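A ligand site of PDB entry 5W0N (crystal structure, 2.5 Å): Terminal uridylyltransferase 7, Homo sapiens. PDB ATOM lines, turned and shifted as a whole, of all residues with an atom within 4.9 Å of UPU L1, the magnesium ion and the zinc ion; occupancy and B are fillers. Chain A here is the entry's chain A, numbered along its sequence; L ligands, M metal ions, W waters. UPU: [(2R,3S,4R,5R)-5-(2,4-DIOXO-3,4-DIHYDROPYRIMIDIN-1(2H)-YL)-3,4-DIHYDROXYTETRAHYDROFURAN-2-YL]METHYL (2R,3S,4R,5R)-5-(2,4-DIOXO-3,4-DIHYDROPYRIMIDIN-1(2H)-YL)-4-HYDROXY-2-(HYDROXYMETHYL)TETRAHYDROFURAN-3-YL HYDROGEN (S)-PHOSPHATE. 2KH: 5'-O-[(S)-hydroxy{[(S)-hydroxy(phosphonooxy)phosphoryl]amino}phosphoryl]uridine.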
ATOM      1  N   PHE A  83      10.533  -1.098 -24.697  1.00  0.00           N
ATOM      2  CA  PHE A  83       9.609  -2.044 -25.315  1.00  0.00           C
ATOM      3  C   PHE A  83       9.283  -3.111 -24.274  1.00  0.00           C
ATOM      4  O   PHE A  83       9.589  -2.961 -23.081  1.00  0.00           O
ATOM      5  CB  PHE A  83      10.203  -2.624 -26.606  1.00  0.00           C
ATOM      6  CG  PHE A  83      11.375  -3.534 -26.405  1.00  0.00           C
ATOM      7  CD1 PHE A  83      12.634  -3.021 -26.151  1.00  0.00           C
ATOM      8  CD2 PHE A  83      11.224  -4.915 -26.507  1.00  0.00           C
ATOM      9  CE1 PHE A  83      13.722  -3.862 -25.982  1.00  0.00           C
ATOM     10  CE2 PHE A  83      12.311  -5.769 -26.335  1.00  0.00           C
ATOM     11  CZ  PHE A  83      13.558  -5.230 -26.070  1.00  0.00           C
ATOM     12  N   SER A  85       6.981  -5.446 -21.738  1.00  0.00           N
ATOM     13  CA  SER A  85       5.796  -5.278 -20.898  1.00  0.00           C
ATOM     14  C   SER A  85       5.712  -3.899 -20.253  1.00  0.00           C
ATOM     15  O   SER A  85       4.643  -3.552 -19.733  1.00  0.00           O
ATOM     16  CB  SER A  85       5.754  -6.354 -19.824  1.00  0.00           C
ATOM     17  OG  SER A  85       6.748  -6.143 -18.838  1.00  0.00           O
ATOM     18  N   ASP A  96      11.207  -6.677 -15.662  1.00  0.00           N
ATOM     19  CA  ASP A  96      12.438  -6.031 -16.101  1.00  0.00           C
ATOM     20  C   ASP A  96      12.111  -4.853 -17.019  1.00  0.00           C
ATOM     21  O   ASP A  96      10.984  -4.653 -17.455  1.00  0.00           O
ATOM     22  CB  ASP A  96      13.353  -7.051 -16.788  1.00  0.00           C
ATOM     23  CG  ASP A  96      12.776  -7.586 -18.093  1.00  0.00           C
ATOM     24  OD1 ASP A  96      11.651  -7.223 -18.441  1.00  0.00           O
ATOM     25  OD2 ASP A  96      13.472  -8.387 -18.757  1.00  0.00           O
ATOM     26  N   ASP A  98      12.928  -3.435 -20.507  1.00  0.00           N
ATOM     27  CA  ASP A  98      13.457  -3.807 -21.806  1.00  0.00           C
ATOM     28  C   ASP A  98      13.716  -2.557 -22.638  1.00  0.00           C
ATOM     29  O   ASP A  98      12.796  -1.775 -22.902  1.00  0.00           O
ATOM     30  CB  ASP A  98      12.490  -4.741 -22.527  1.00  0.00           C
ATOM     31  CG  ASP A  98      12.191  -5.977 -21.733  1.00  0.00           C
ATOM     32  OD1 ASP A  98      13.085  -6.832 -21.614  1.00  0.00           O
ATOM     33  OD2 ASP A  98      11.058  -6.101 -21.211  1.00  0.00           O
ATOM     34  N   ILE A 137      25.771 -10.312 -22.482  1.00  0.00           N
ATOM     35  CA  ILE A 137      25.450 -11.669 -22.923  1.00  0.00           C
ATOM     36  C   ILE A 137      25.431 -11.619 -24.451  1.00  0.00           C
ATOM     37  O   ILE A 137      24.407 -11.373 -25.077  1.00  0.00           O
ATOM     38  CB  ILE A 137      24.122 -12.172 -22.358  1.00  0.00           C
ATOM     39  CG1 ILE A 137      24.142 -12.067 -20.823  1.00  0.00           C
ATOM     40  CG2 ILE A 137      23.848 -13.608 -22.809  1.00  0.00           C
ATOM     41  CD1 ILE A 137      22.865 -12.535 -20.138  1.00  0.00           C
ATOM     42  N   THR A 139      26.360 -14.128 -26.606  1.00  0.00           N
ATOM     43  CA  THR A 139      26.140 -15.396 -27.297  1.00  0.00           C
ATOM     44  C   THR A 139      24.664 -15.724 -27.489  1.00  0.00           C
ATOM     45  O   THR A 139      24.351 -16.696 -28.190  1.00  0.00           O
ATOM     46  CB  THR A 139      26.806 -16.537 -26.514  1.00  0.00           C
ATOM     47  OG1 THR A 139      26.221 -16.652 -25.214  1.00  0.00           O
ATOM     48  CG2 THR A 139      28.306 -16.295 -26.393  1.00  0.00           C
ATOM     49  N   ALA A 140      23.758 -14.952 -26.902  1.00  0.00           N
ATOM     50  CA  ALA A 140      22.330 -15.214 -27.054  1.00  0.00           C
ATOM     51  C   ALA A 140      21.863 -14.827 -28.448  1.00  0.00           C
ATOM     52  O   ALA A 140      22.486 -14.020 -29.147  1.00  0.00           O
ATOM     53  CB  ALA A 140      21.528 -14.449 -25.999  1.00  0.00           C
ATOM     54  N   LYS A 141      20.740 -15.422 -28.867  1.00  0.00           N
ATOM     55  CA  LYS A 141      20.126 -15.047 -30.146  1.00  0.00           C
ATOM     56  C   LYS A 141      19.986 -13.532 -30.245  1.00  0.00           C
ATOM     57  O   LYS A 141      20.329 -12.924 -31.268  1.00  0.00           O
ATOM     58  CB  LYS A 141      18.768 -15.714 -30.290  1.00  0.00           C
ATOM     59  CG  LYS A 141      18.803 -17.190 -30.649  1.00  0.00           C
ATOM     60  CD  LYS A 141      17.422 -17.818 -30.511  1.00  0.00           C
ATOM     61  CE  LYS A 141      17.441 -19.314 -30.788  1.00  0.00           C
ATOM     62  NZ  LYS A 141      17.659 -19.617 -32.236  1.00  0.00           N
ATOM     63  N   VAL A 142      19.495 -12.910 -29.184  1.00  0.00           N
ATOM     64  CA  VAL A 142      19.434 -11.455 -29.074  1.00  0.00           C
ATOM     65  C   VAL A 142      20.492 -11.020 -28.059  1.00  0.00           C
ATOM     66  O   VAL A 142      20.242 -11.072 -26.848  1.00  0.00           O
ATOM     67  CB  VAL A 142      18.043 -10.978 -28.642  1.00  0.00           C
ATOM     68  CG1 VAL A 142      18.014  -9.457 -28.498  1.00  0.00           C
ATOM     69  CG2 VAL A 142      16.998 -11.452 -29.638  1.00  0.00           C
ATOM     70  N   ILE A 144      22.474  -8.994 -25.430  1.00  0.00           N
ATOM     71  CA  ILE A 144      22.060  -7.928 -24.525  1.00  0.00           C
ATOM     72  C   ILE A 144      23.198  -7.598 -23.577  1.00  0.00           C
ATOM     73  O   ILE A 144      24.153  -8.362 -23.406  1.00  0.00           O
ATOM     74  CB  ILE A 144      20.803  -8.298 -23.714  1.00  0.00           C
ATOM     75  CG1 ILE A 144      21.005  -9.658 -23.015  1.00  0.00           C
ATOM     76  CG2 ILE A 144      19.581  -8.313 -24.599  1.00  0.00           C
ATOM     77  CD1 ILE A 144      19.947  -9.994 -22.003  1.00  0.00           C
ATOM     78  N   ASP A 157      17.564  -4.597 -19.403  1.00  0.00           N
ATOM     79  CA  ASP A 157      18.141  -5.360 -20.508  1.00  0.00           C
ATOM     80  C   ASP A 157      18.170  -4.479 -21.740  1.00  0.00           C
ATOM     81  O   ASP A 157      17.111  -4.091 -22.252  1.00  0.00           O
ATOM     82  CB  ASP A 157      17.319  -6.622 -20.797  1.00  0.00           C
ATOM     83  CG  ASP A 157      17.289  -7.601 -19.634  1.00  0.00           C
ATOM     84  OD1 ASP A 157      17.020  -7.179 -18.493  1.00  0.00           O
ATOM     85  OD2 ASP A 157      17.532  -8.801 -19.869  1.00  0.00           O
ATOM     86  N   SER A 159      19.220  -4.042 -25.692  1.00  0.00           N
ATOM     87  CA  SER A 159      19.535  -4.725 -26.944  1.00  0.00           C
ATOM     88  C   SER A 159      19.715  -3.688 -28.050  1.00  0.00           C
ATOM     89  O   SER A 159      19.271  -2.541 -27.926  1.00  0.00           O
ATOM     90  CB  SER A 159      18.441  -5.735 -27.320  1.00  0.00           C
ATOM     91  OG  SER A 159      17.149  -5.133 -27.303  1.00  0.00           O
ATOM     92  N   ASN A 162      16.706  -3.686 -31.991  1.00  0.00           N
ATOM     93  CA  ASN A 162      15.673  -4.705 -31.831  1.00  0.00           C
ATOM     94  C   ASN A 162      14.363  -4.167 -32.393  1.00  0.00           C
ATOM     95  O   ASN A 162      13.370  -3.970 -31.700  1.00  0.00           O
ATOM     96  CB  ASN A 162      15.545  -5.083 -30.359  1.00  0.00           C
ATOM     97  CG  ASN A 162      14.918  -6.432 -30.157  1.00  0.00           C
ATOM     98  OD1 ASN A 162      14.301  -6.991 -31.063  1.00  0.00           O
ATOM     99  ND2 ASN A 162      15.070  -6.968 -28.960  1.00  0.00           N
ATOM    100  N   ALA A 165      10.988  -6.128 -32.136  1.00  0.00           N
ATOM    101  CA  ALA A 165      10.438  -6.152 -30.786  1.00  0.00           C
ATOM    102  C   ALA A 165       9.614  -4.896 -30.509  1.00  0.00           C
ATOM    103  O   ALA A 165       8.566  -4.955 -29.859  1.00  0.00           O
ATOM    104  CB  ALA A 165      11.555  -6.290 -29.761  1.00  0.00           C
ATOM    105  N   ASP A 200      10.356 -18.656 -17.895  1.00  0.00           N
ATOM    106  CA  ASP A 200      11.720 -18.131 -17.982  1.00  0.00           C
ATOM    107  C   ASP A 200      12.462 -18.876 -19.089  1.00  0.00           C
ATOM    108  O   ASP A 200      12.990 -19.969 -18.848  1.00  0.00           O
ATOM    109  CB  ASP A 200      12.440 -18.270 -16.644  1.00  0.00           C
ATOM    110  CG  ASP A 200      13.726 -17.483 -16.593  1.00  0.00           C
ATOM    111  OD1 ASP A 200      14.230 -17.076 -17.667  1.00  0.00           O
ATOM    112  OD2 ASP A 200      14.243 -17.287 -15.478  1.00  0.00           O
ATOM    113  N   ALA A 201      12.540 -18.260 -20.258  1.00  0.00           N
ATOM    114  CA  ALA A 201      13.226 -18.897 -21.381  1.00  0.00           C
ATOM    115  C   ALA A 201      14.713 -19.100 -21.092  1.00  0.00           C
ATOM    116  O   ALA A 201      15.331 -20.019 -21.641  1.00  0.00           O
ATOM    117  CB  ALA A 201      13.036 -18.071 -22.655  1.00  0.00           C
ATOM    118  N   SER A 202      15.302 -18.254 -20.243  1.00  0.00           N
ATOM    119  CA  SER A 202      16.706 -18.413 -19.889  1.00  0.00           C
ATOM    120  C   SER A 202      16.957 -19.633 -19.008  1.00  0.00           C
ATOM    121  O   SER A 202      18.118 -20.004 -18.822  1.00  0.00           O
ATOM    122  CB  SER A 202      17.214 -17.151 -19.177  1.00  0.00           C
ATOM    123  OG  SER A 202      16.666 -17.041 -17.875  1.00  0.00           O
ATOM    124  N   HIS A 324      10.565 -17.669 -36.563  1.00  0.00           N
ATOM    125  CA  HIS A 324      10.861 -17.825 -35.143  1.00  0.00           C
ATOM    126  C   HIS A 324       9.755 -18.651 -34.495  1.00  0.00           C
ATOM    127  O   HIS A 324       8.600 -18.223 -34.438  1.00  0.00           O
ATOM    128  CB  HIS A 324      10.987 -16.466 -34.468  1.00  0.00           C
ATOM    129  CG  HIS A 324      11.412 -16.546 -33.034  1.00  0.00           C
ATOM    130  ND1 HIS A 324      11.944 -17.693 -32.472  1.00  0.00           N
ATOM    131  CD2 HIS A 324      11.378 -15.627 -32.037  1.00  0.00           C
ATOM    132  CE1 HIS A 324      12.225 -17.471 -31.204  1.00  0.00           C
ATOM    133  NE2 HIS A 324      11.883 -16.227 -30.911  1.00  0.00           N
ATOM    134  N   CYS A 385      22.985 -24.546 -16.614  1.00  0.00           N
ATOM    135  CA  CYS A 385      24.243 -24.553 -15.888  1.00  0.00           C
ATOM    136  C   CYS A 385      24.001 -24.910 -14.420  1.00  0.00           C
ATOM    137  O   CYS A 385      23.030 -24.450 -13.808  1.00  0.00           O
ATOM    138  CB  CYS A 385      24.920 -23.185 -16.006  1.00  0.00           C
ATOM    139  SG  CYS A 385      26.379 -22.933 -14.973  1.00  0.00           S
ATOM    140  N   ILE A 387      25.718 -24.009 -11.924  1.00  0.00           N
ATOM    141  CA  ILE A 387      26.141 -22.952 -11.014  1.00  0.00           C
ATOM    142  C   ILE A 387      25.057 -21.896 -10.838  1.00  0.00           C
ATOM    143  O   ILE A 387      24.696 -21.544  -9.711  1.00  0.00           O
ATOM    144  CB  ILE A 387      27.459 -22.329 -11.516  1.00  0.00           C
ATOM    145  CG1 ILE A 387      28.548 -23.401 -11.616  1.00  0.00           C
ATOM    146  CG2 ILE A 387      27.898 -21.193 -10.609  1.00  0.00           C
ATOM    147  CD1 ILE A 387      29.838 -22.924 -12.261  1.00  0.00           C
ATOM    148  N   CYS A 388      24.522 -21.378 -11.945  1.00  0.00           N
ATOM    149  CA  CYS A 388      23.554 -20.299 -11.903  1.00  0.00           C
ATOM    150  C   CYS A 388      22.145 -20.720 -12.316  1.00  0.00           C
ATOM    151  O   CYS A 388      21.186 -20.036 -11.938  1.00  0.00           O
ATOM    152  CB  CYS A 388      23.997 -19.139 -12.808  1.00  0.00           C
ATOM    153  SG  CYS A 388      24.020 -19.555 -14.566  1.00  0.00           S
ATOM    154  N   GLY A 389      22.001 -21.810 -13.066  1.00  0.00           N
ATOM    155  CA  GLY A 389      20.700 -22.259 -13.503  1.00  0.00           C
ATOM    156  C   GLY A 389      20.234 -21.678 -14.825  1.00  0.00           C
ATOM    157  O   GLY A 389      19.059 -21.845 -15.166  1.00  0.00           O
ATOM    158  N   LYS A 390      21.114 -21.023 -15.567  1.00  0.00           N
ATOM    159  CA  LYS A 390      20.793 -20.461 -16.870  1.00  0.00           C
ATOM    160  C   LYS A 390      21.315 -21.368 -17.977  1.00  0.00           C
ATOM    161  O   LYS A 390      22.249 -22.151 -17.772  1.00  0.00           O
ATOM    162  CB  LYS A 390      21.377 -19.052 -17.026  1.00  0.00           C
ATOM    163  CG  LYS A 390      20.892 -18.037 -16.000  1.00  0.00           C
ATOM    164  CD  LYS A 390      19.387 -17.811 -16.098  1.00  0.00           C
ATOM    165  CE  LYS A 390      18.954 -16.563 -15.340  1.00  0.00           C
ATOM    166  NZ  LYS A 390      19.406 -15.318 -16.010  1.00  0.00           N
ATOM    167  N   ILE A 391      20.718 -21.237 -19.152  1.00  0.00           N
ATOM    168  CA  ILE A 391      21.137 -21.991 -20.316  1.00  0.00           C
ATOM    169  C   ILE A 391      22.063 -21.124 -21.159  1.00  0.00           C
ATOM    170  O   ILE A 391      22.121 -19.903 -21.016  1.00  0.00           O
ATOM    171  CB  ILE A 391      19.924 -22.477 -21.150  1.00  0.00           C
ATOM    172  CG1 ILE A 391      19.121 -21.293 -21.692  1.00  0.00           C
ATOM    173  CG2 ILE A 391      19.029 -23.392 -20.315  1.00  0.00           C
ATOM    174  CD1 ILE A 391      19.458 -20.917 -23.121  1.00  0.00           C
ATOM    175  N   GLY A 392      22.816 -21.776 -22.050  1.00  0.00           N
ATOM    176  CA  GLY A 392      23.564 -21.076 -23.068  1.00  0.00           C
ATOM    177  C   GLY A 392      25.021 -20.779 -22.773  1.00  0.00           C
ATOM    178  O   GLY A 392      25.592 -19.896 -23.424  1.00  0.00           O
ATOM    179  N   HIS A 393      25.642 -21.469 -21.823  1.00  0.00           N
ATOM    180  CA  HIS A 393      27.049 -21.233 -21.552  1.00  0.00           C
ATOM    181  C   HIS A 393      27.642 -22.420 -20.799  1.00  0.00           C
ATOM    182  O   HIS A 393      26.957 -23.096 -20.034  1.00  0.00           O
ATOM    183  CB  HIS A 393      27.270 -19.940 -20.742  1.00  0.00           C
ATOM    184  CG  HIS A 393      26.793 -20.023 -19.321  1.00  0.00           C
ATOM    185  ND1 HIS A 393      25.682 -19.362 -18.872  1.00  0.00           N
ATOM    186  CD2 HIS A 393      27.298 -20.690 -18.255  1.00  0.00           C
ATOM    187  CE1 HIS A 393      25.504 -19.610 -17.584  1.00  0.00           C
ATOM    188  NE2 HIS A 393      26.472 -20.410 -17.185  1.00  0.00           N
ATOM    189  N   CYS A 398      30.556 -19.071 -16.736  1.00  0.00           N
ATOM    190  CA  CYS A 398      29.461 -18.699 -15.853  1.00  0.00           C
ATOM    191  C   CYS A 398      29.814 -17.436 -15.065  1.00  0.00           C
ATOM    192  O   CYS A 398      30.937 -17.320 -14.547  1.00  0.00           O
ATOM    193  CB  CYS A 398      29.145 -19.839 -14.894  1.00  0.00           C
ATOM    194  SG  CYS A 398      27.697 -19.570 -13.852  1.00  0.00           S
ATOM    195  N   PRO A 399      28.897 -16.466 -14.953  1.00  0.00           N
ATOM    196  CA  PRO A 399      29.194 -15.307 -14.100  1.00  0.00           C
ATOM    197  C   PRO A 399      29.309 -15.648 -12.623  1.00  0.00           C
ATOM    198  O   PRO A 399      30.169 -15.088 -11.930  1.00  0.00           O
ATOM    199  CB  PRO A 399      28.005 -14.368 -14.364  1.00  0.00           C
ATOM    200  CG  PRO A 399      27.448 -14.802 -15.671  1.00  0.00           C
ATOM    201  CD  PRO A 399      27.667 -16.285 -15.736  1.00  0.00           C
HETATM  202  O2A UPU L   1      14.423  -8.396 -27.015  1.00  0.00           O
HETATM  203  C2A UPU L   1      14.439  -9.611 -27.002  1.00  0.00           C
HETATM  204  N3A UPU L   1      13.880 -10.402 -28.134  1.00  0.00           N
HETATM  205  C4A UPU L   1      13.915 -11.855 -28.104  1.00  0.00           C
HETATM  206  O4A UPU L   1      13.471 -12.476 -29.007  1.00  0.00           O
HETATM  207  C5A UPU L   1      14.513 -12.573 -26.931  1.00  0.00           C
HETATM  208  C6A UPU L   1      15.076 -11.787 -25.792  1.00  0.00           C
HETATM  209  N1A UPU L   1      15.039 -10.315 -25.834  1.00  0.00           N
HETATM  210 C1'A UPU L   1      15.570  -9.534 -24.749  1.00  0.00           C
HETATM  211 O4'A UPU L   1      16.641 -10.423 -23.939  1.00  0.00           O
HETATM  212 C2'A UPU L   1      14.617  -9.198 -23.910  1.00  0.00           C
HETATM  213 O2'A UPU L   1      14.793  -7.790 -23.478  1.00  0.00           O
HETATM  214 C3'A UPU L   1      14.772 -10.134 -22.701  1.00  0.00           C
HETATM  215 O3'A UPU L   1      14.362  -9.510 -21.555  1.00  0.00           O
HETATM  216 C4'A UPU L   1      16.283 -10.396 -22.682  1.00  0.00           C
HETATM  217 C5'A UPU L   1      16.567 -11.801 -22.048  1.00  0.00           C
HETATM  218 O5'A UPU L   1      15.819 -12.732 -22.816  1.00  0.00           O
HETATM  219  P   UPU L   1      15.470 -14.225 -22.118  1.00  0.00           P
HETATM  220  O1  UPU L   1      14.875 -14.032 -20.764  1.00  0.00           O
HETATM  221  O2  UPU L   1      14.519 -14.939 -23.000  1.00  0.00           O
HETATM  222 O3'B UPU L   1      16.891 -15.057 -22.001  1.00  0.00           O
HETATM  223 C3'B UPU L   1      17.749 -15.257 -23.234  1.00  0.00           C
HETATM  224 C4'B UPU L   1      17.726 -16.792 -23.612  1.00  0.00           C
HETATM  225 C5'B UPU L   1      18.163 -17.028 -24.920  1.00  0.00           C
HETATM  226 O5'B UPU L   1      17.053 -16.844 -25.825  1.00  0.00           O
HETATM  227 O4'B UPU L   1      18.674 -17.401 -22.606  1.00  0.00           O
HETATM  228 C2'B UPU L   1      18.927 -15.084 -22.954  1.00  0.00           C
HETATM  229 O2'B UPU L   1      19.141 -13.830 -22.182  1.00  0.00           O
HETATM  230 C1'B UPU L   1      19.253 -16.418 -22.017  1.00  0.00           C
HETATM  231  N1B UPU L   1      20.677 -16.658 -21.934  1.00  0.00           N
HETATM  232  C2B UPU L   1      21.360 -16.504 -20.606  1.00  0.00           C
HETATM  233  O2B UPU L   1      20.710 -16.175 -19.636  1.00  0.00           O
HETATM  234  C6B UPU L   1      21.448 -17.059 -23.120  1.00  0.00           C
HETATM  235  C5B UPU L   1      22.912 -17.314 -22.999  1.00  0.00           C
HETATM  236  C4B UPU L   1      23.603 -17.158 -21.659  1.00  0.00           C
HETATM  237  N3B UPU L   1      22.816 -16.757 -20.481  1.00  0.00           N
HETATM  238  O4B UPU L   1      24.771 -17.345 -21.553  1.00  0.00           O
HETATM  239  PA  2KH L   2      10.552 -10.306 -21.821  1.00  0.00           P
HETATM  240  O1A 2KH L   2      11.281 -11.615 -21.492  1.00  0.00           O
HETATM  241  O2A 2KH L   2      10.989  -9.240 -20.847  1.00  0.00           O
HETATM  242  N3A 2KH L   2       8.842 -10.548 -21.691  1.00  0.00           N
HETATM  243  O5' 2KH L   2      10.918  -9.810 -23.370  1.00  0.00           O
HETATM  244  PB  2KH L   2       7.828  -9.227 -21.383  1.00  0.00           P
HETATM  245  O1B 2KH L   2       8.667  -7.976 -21.185  1.00  0.00           O
HETATM  246  O2B 2KH L   2       6.891  -9.044 -22.500  1.00  0.00           O
HETATM  247  O3B 2KH L   2       6.998  -9.523 -19.995  1.00  0.00           O
HETATM  248  PG  2KH L   2       7.688  -9.462 -18.492  1.00  0.00           P
HETATM  249  O1G 2KH L   2       6.759  -8.739 -17.569  1.00  0.00           O
HETATM  250  O2G 2KH L   2       7.944 -10.853 -17.978  1.00  0.00           O
HETATM  251  O3G 2KH L   2       9.016  -8.709 -18.584  1.00  0.00           O
HETATM  252  C5' 2KH L   2      10.686  -8.430 -23.669  1.00  0.00           C
HETATM  253  C4' 2KH L   2      10.149  -8.241 -25.136  1.00  0.00           C
HETATM  254  O4' 2KH L   2      11.199  -8.774 -26.166  1.00  0.00           O
HETATM  255  C1' 2KH L   2      10.361  -9.249 -27.336  1.00  0.00           C
HETATM  256  C2' 2KH L   2       9.100  -9.010 -26.996  1.00  0.00           C
HETATM  257  O2' 2KH L   2       8.671  -7.718 -27.535  1.00  0.00           O
HETATM  258  C3' 2KH L   2       9.107  -8.950 -25.385  1.00  0.00           C
HETATM  259  O3' 2KH L   2       7.871  -8.289 -24.911  1.00  0.00           O
HETATM  260  N1  2KH L   2      10.559 -10.733 -27.522  1.00  0.00           N
HETATM  261  C6  2KH L   2      10.878 -11.575 -26.389  1.00  0.00           C
HETATM  262  C2  2KH L   2      10.434 -11.323 -28.893  1.00  0.00           C
HETATM  263  O2  2KH L   2      10.186 -10.631 -29.799  1.00  0.00           O
HETATM  264  N3  2KH L   2      10.630 -12.789 -29.090  1.00  0.00           N
HETATM  265  C4  2KH L   2      10.948 -13.644 -27.954  1.00  0.00           C
HETATM  266  O4  2KH L   2      11.111 -14.805 -28.117  1.00  0.00           O
HETATM  267  C5  2KH L   2      11.077 -13.046 -26.580  1.00  0.00           C
HETATM  268 MG    MG M   1      10.287  -7.600 -19.949  1.00  0.00          MG
HETATM  269 ZN    ZN M   2      26.048 -20.515 -15.195  1.00  0.00          ZN
HETATM  270  O   HOH W   1      18.927 -13.246 -19.507  1.00  0.00           O
HETATM  271  O   HOH W   2      13.998 -16.011 -25.787  1.00  0.00           O
HETATM  272  O   HOH W   3      16.431  -5.708 -24.509  1.00  0.00           O
HETATM  273  O   HOH W   4      11.839 -13.377 -23.216  1.00  0.00           O
HETATM  274  O   HOH W   5      12.280 -15.559 -20.502  1.00  0.00           O
HETATM  275  O   HOH W   6      18.162 -14.248 -26.874  1.00  0.00           O
HETATM  276  O   HOH W   7      18.808 -12.216 -24.966  1.00  0.00           O
HETATM  277  O   HOH W   8      13.253 -11.969 -19.907  1.00  0.00           O
HETATM  278  O   HOH W   9      15.014 -15.280 -28.861  1.00  0.00           O
HETATM  279  O   HOH W  10      21.335 -14.048 -17.654  1.00  0.00           O
HETATM  280  O   HOH W  11       9.363  -5.940 -19.334  1.00  0.00           O
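The zinc ion is bound by NE2 of His 393 (2.0 Å), SG of Cys 398 (2.3 Å), SG of Cys 388 (2.3 Å) and SG of Cys 385 (2.5 Å).
An oxygen (O4A) of UPU L1 sits at hydrogen-bond distance from a nitrogen (N3) of 2KH L2 (2.9 Å).
O4B of UPU L1 sits close to O of Gly 392 (3.3 Å). Merely in contact with UPU L1: Phe 83, Ile 137, Thr 139, Ala 140, Val 142, Ile 144, Asp 157, Ala 201, Ser 202 and Lys 390. Hydrophobic or aromatic side chains that line UPU L1: Phe 83, Ile 137, Ala 140, Val 142, Ile 144, Ala 201, Ile 391 and His 393. Of the 28 residues printed, 16 come within 4 Å of UPU L1.
A ring nitrogen (ND1) of His 393 lies within hydrogen-bond range of an oxygen (O4B) of UPU L1, 3.5 Å away. The side-chain hydroxyl of Ser 85 lies within hydrogen-bond range of an oxygen (O1G) of 2KH L2 (2.9 Å). The backbone carbonyl oxygen (O) of Ile 391 lies close to a nitrogen (N3B) of UPU L1 (3.3 Å). An oxygen (O2'A) of UPU L1 is in hydrogen-bond range of the side-chain carboxylate (OD1) of Asp 98, 2.7 Å away. O3'A of UPU L1 lies within hydrogen-bond range of OD2 of Asp 96 (3.1 Å). The backbone NH (N) of Ser 85 lies close to an oxygen (O1B) of 2KH L2 (3.1 Å). O4 of 2KH L2 sits at hydrogen-bond distance from NE2 of His 324. The side-chain amide nitrogen of Asn 162 sits at hydrogen-bond distance from an oxygen (O2A) of UPU L1 (2.5 Å).
Water W11 binds the magnesium ion (2.0 Å). The magnesium ion is bound by O2A of 2KH L2. The magnesium ion is bound by OD1 of Asp 96, 2.1 Å away. O1B of 2KH L2 is bound to the magnesium ion, at 2.1 Å. OD2 of Asp 98 binds the magnesium ion (2.1 Å). O3G of 2KH L2 is bound to the magnesium ion (2.2 Å).
O of Asp 98 sits at hydrogen-bond distance from N of Phe 83. ND2 of Asn 162 is in hydrogen-bond range of OG of Ser 159, 3.2 Å away. The backbone NH (N) of Lys 390 lies close to the side-chain sulfur (SG) of Cys 388 (3.4 Å). The backbone NH (N) of Ile 137 lies within hydrogen-bond range of the backbone carbonyl oxygen (O) of Ile 144 (2.7 Å). The side-chain carboxylate (OD1) of Asp 200 sits at hydrogen-bond distance from the side-chain hydroxyl (OG) of Ser 202. The backbone NH of Ile 387 sits close to the side-chain sulfur of Cys 385 (3.3 Å). The backbone NH (N) of Cys 385 is in hydrogen-bond range of the backbone carbonyl oxygen (O) of Lys 390 (2.8 Å). O of Ser 202 lies within hydrogen-bond range of N of Ile 391.
Water W8 lies within hydrogen-bond range of an oxygen (O1A) of 2KH L2 (2.6 Å) and an oxygen (O1) of UPU L1 (2.8 Å). Water W3 lies within hydrogen-bond range of O2'A of UPU L1 (2.8 Å), O of Asp 157 (2.9 Å) and OG of Ser 159 (2.9 Å). Water W10 lies within hydrogen-bond range of NZ of Lys 390 (2.8 Å) and O2B of UPU L1 (3.0 Å). Water W7 lies within hydrogen-bond range of the backbone carbonyl oxygen (O) of Val 142 (2.6 Å) and an oxygen (O4'A) of UPU L1 (3.0 Å). Water W6 lies within hydrogen-bond range of the backbone NH of Val 142 (3.0 Å), an oxygen (O5'B) of UPU L1 (3.0 Å) and the backbone NH of Lys 141 (3.5 Å). Water W4 lies within hydrogen-bond range of O1A of 2KH L2 (2.5 Å) and O2 of UPU L1 (3.1 Å).
Ser 85 touches the magnesium ion (OG to MG, 3.99 Å). Of the 28 residues printed, 3 come within 4 Å of the magnesium ion. Along chain A the residues within 4 Å of the magnesium ion span positions 85 to 98.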
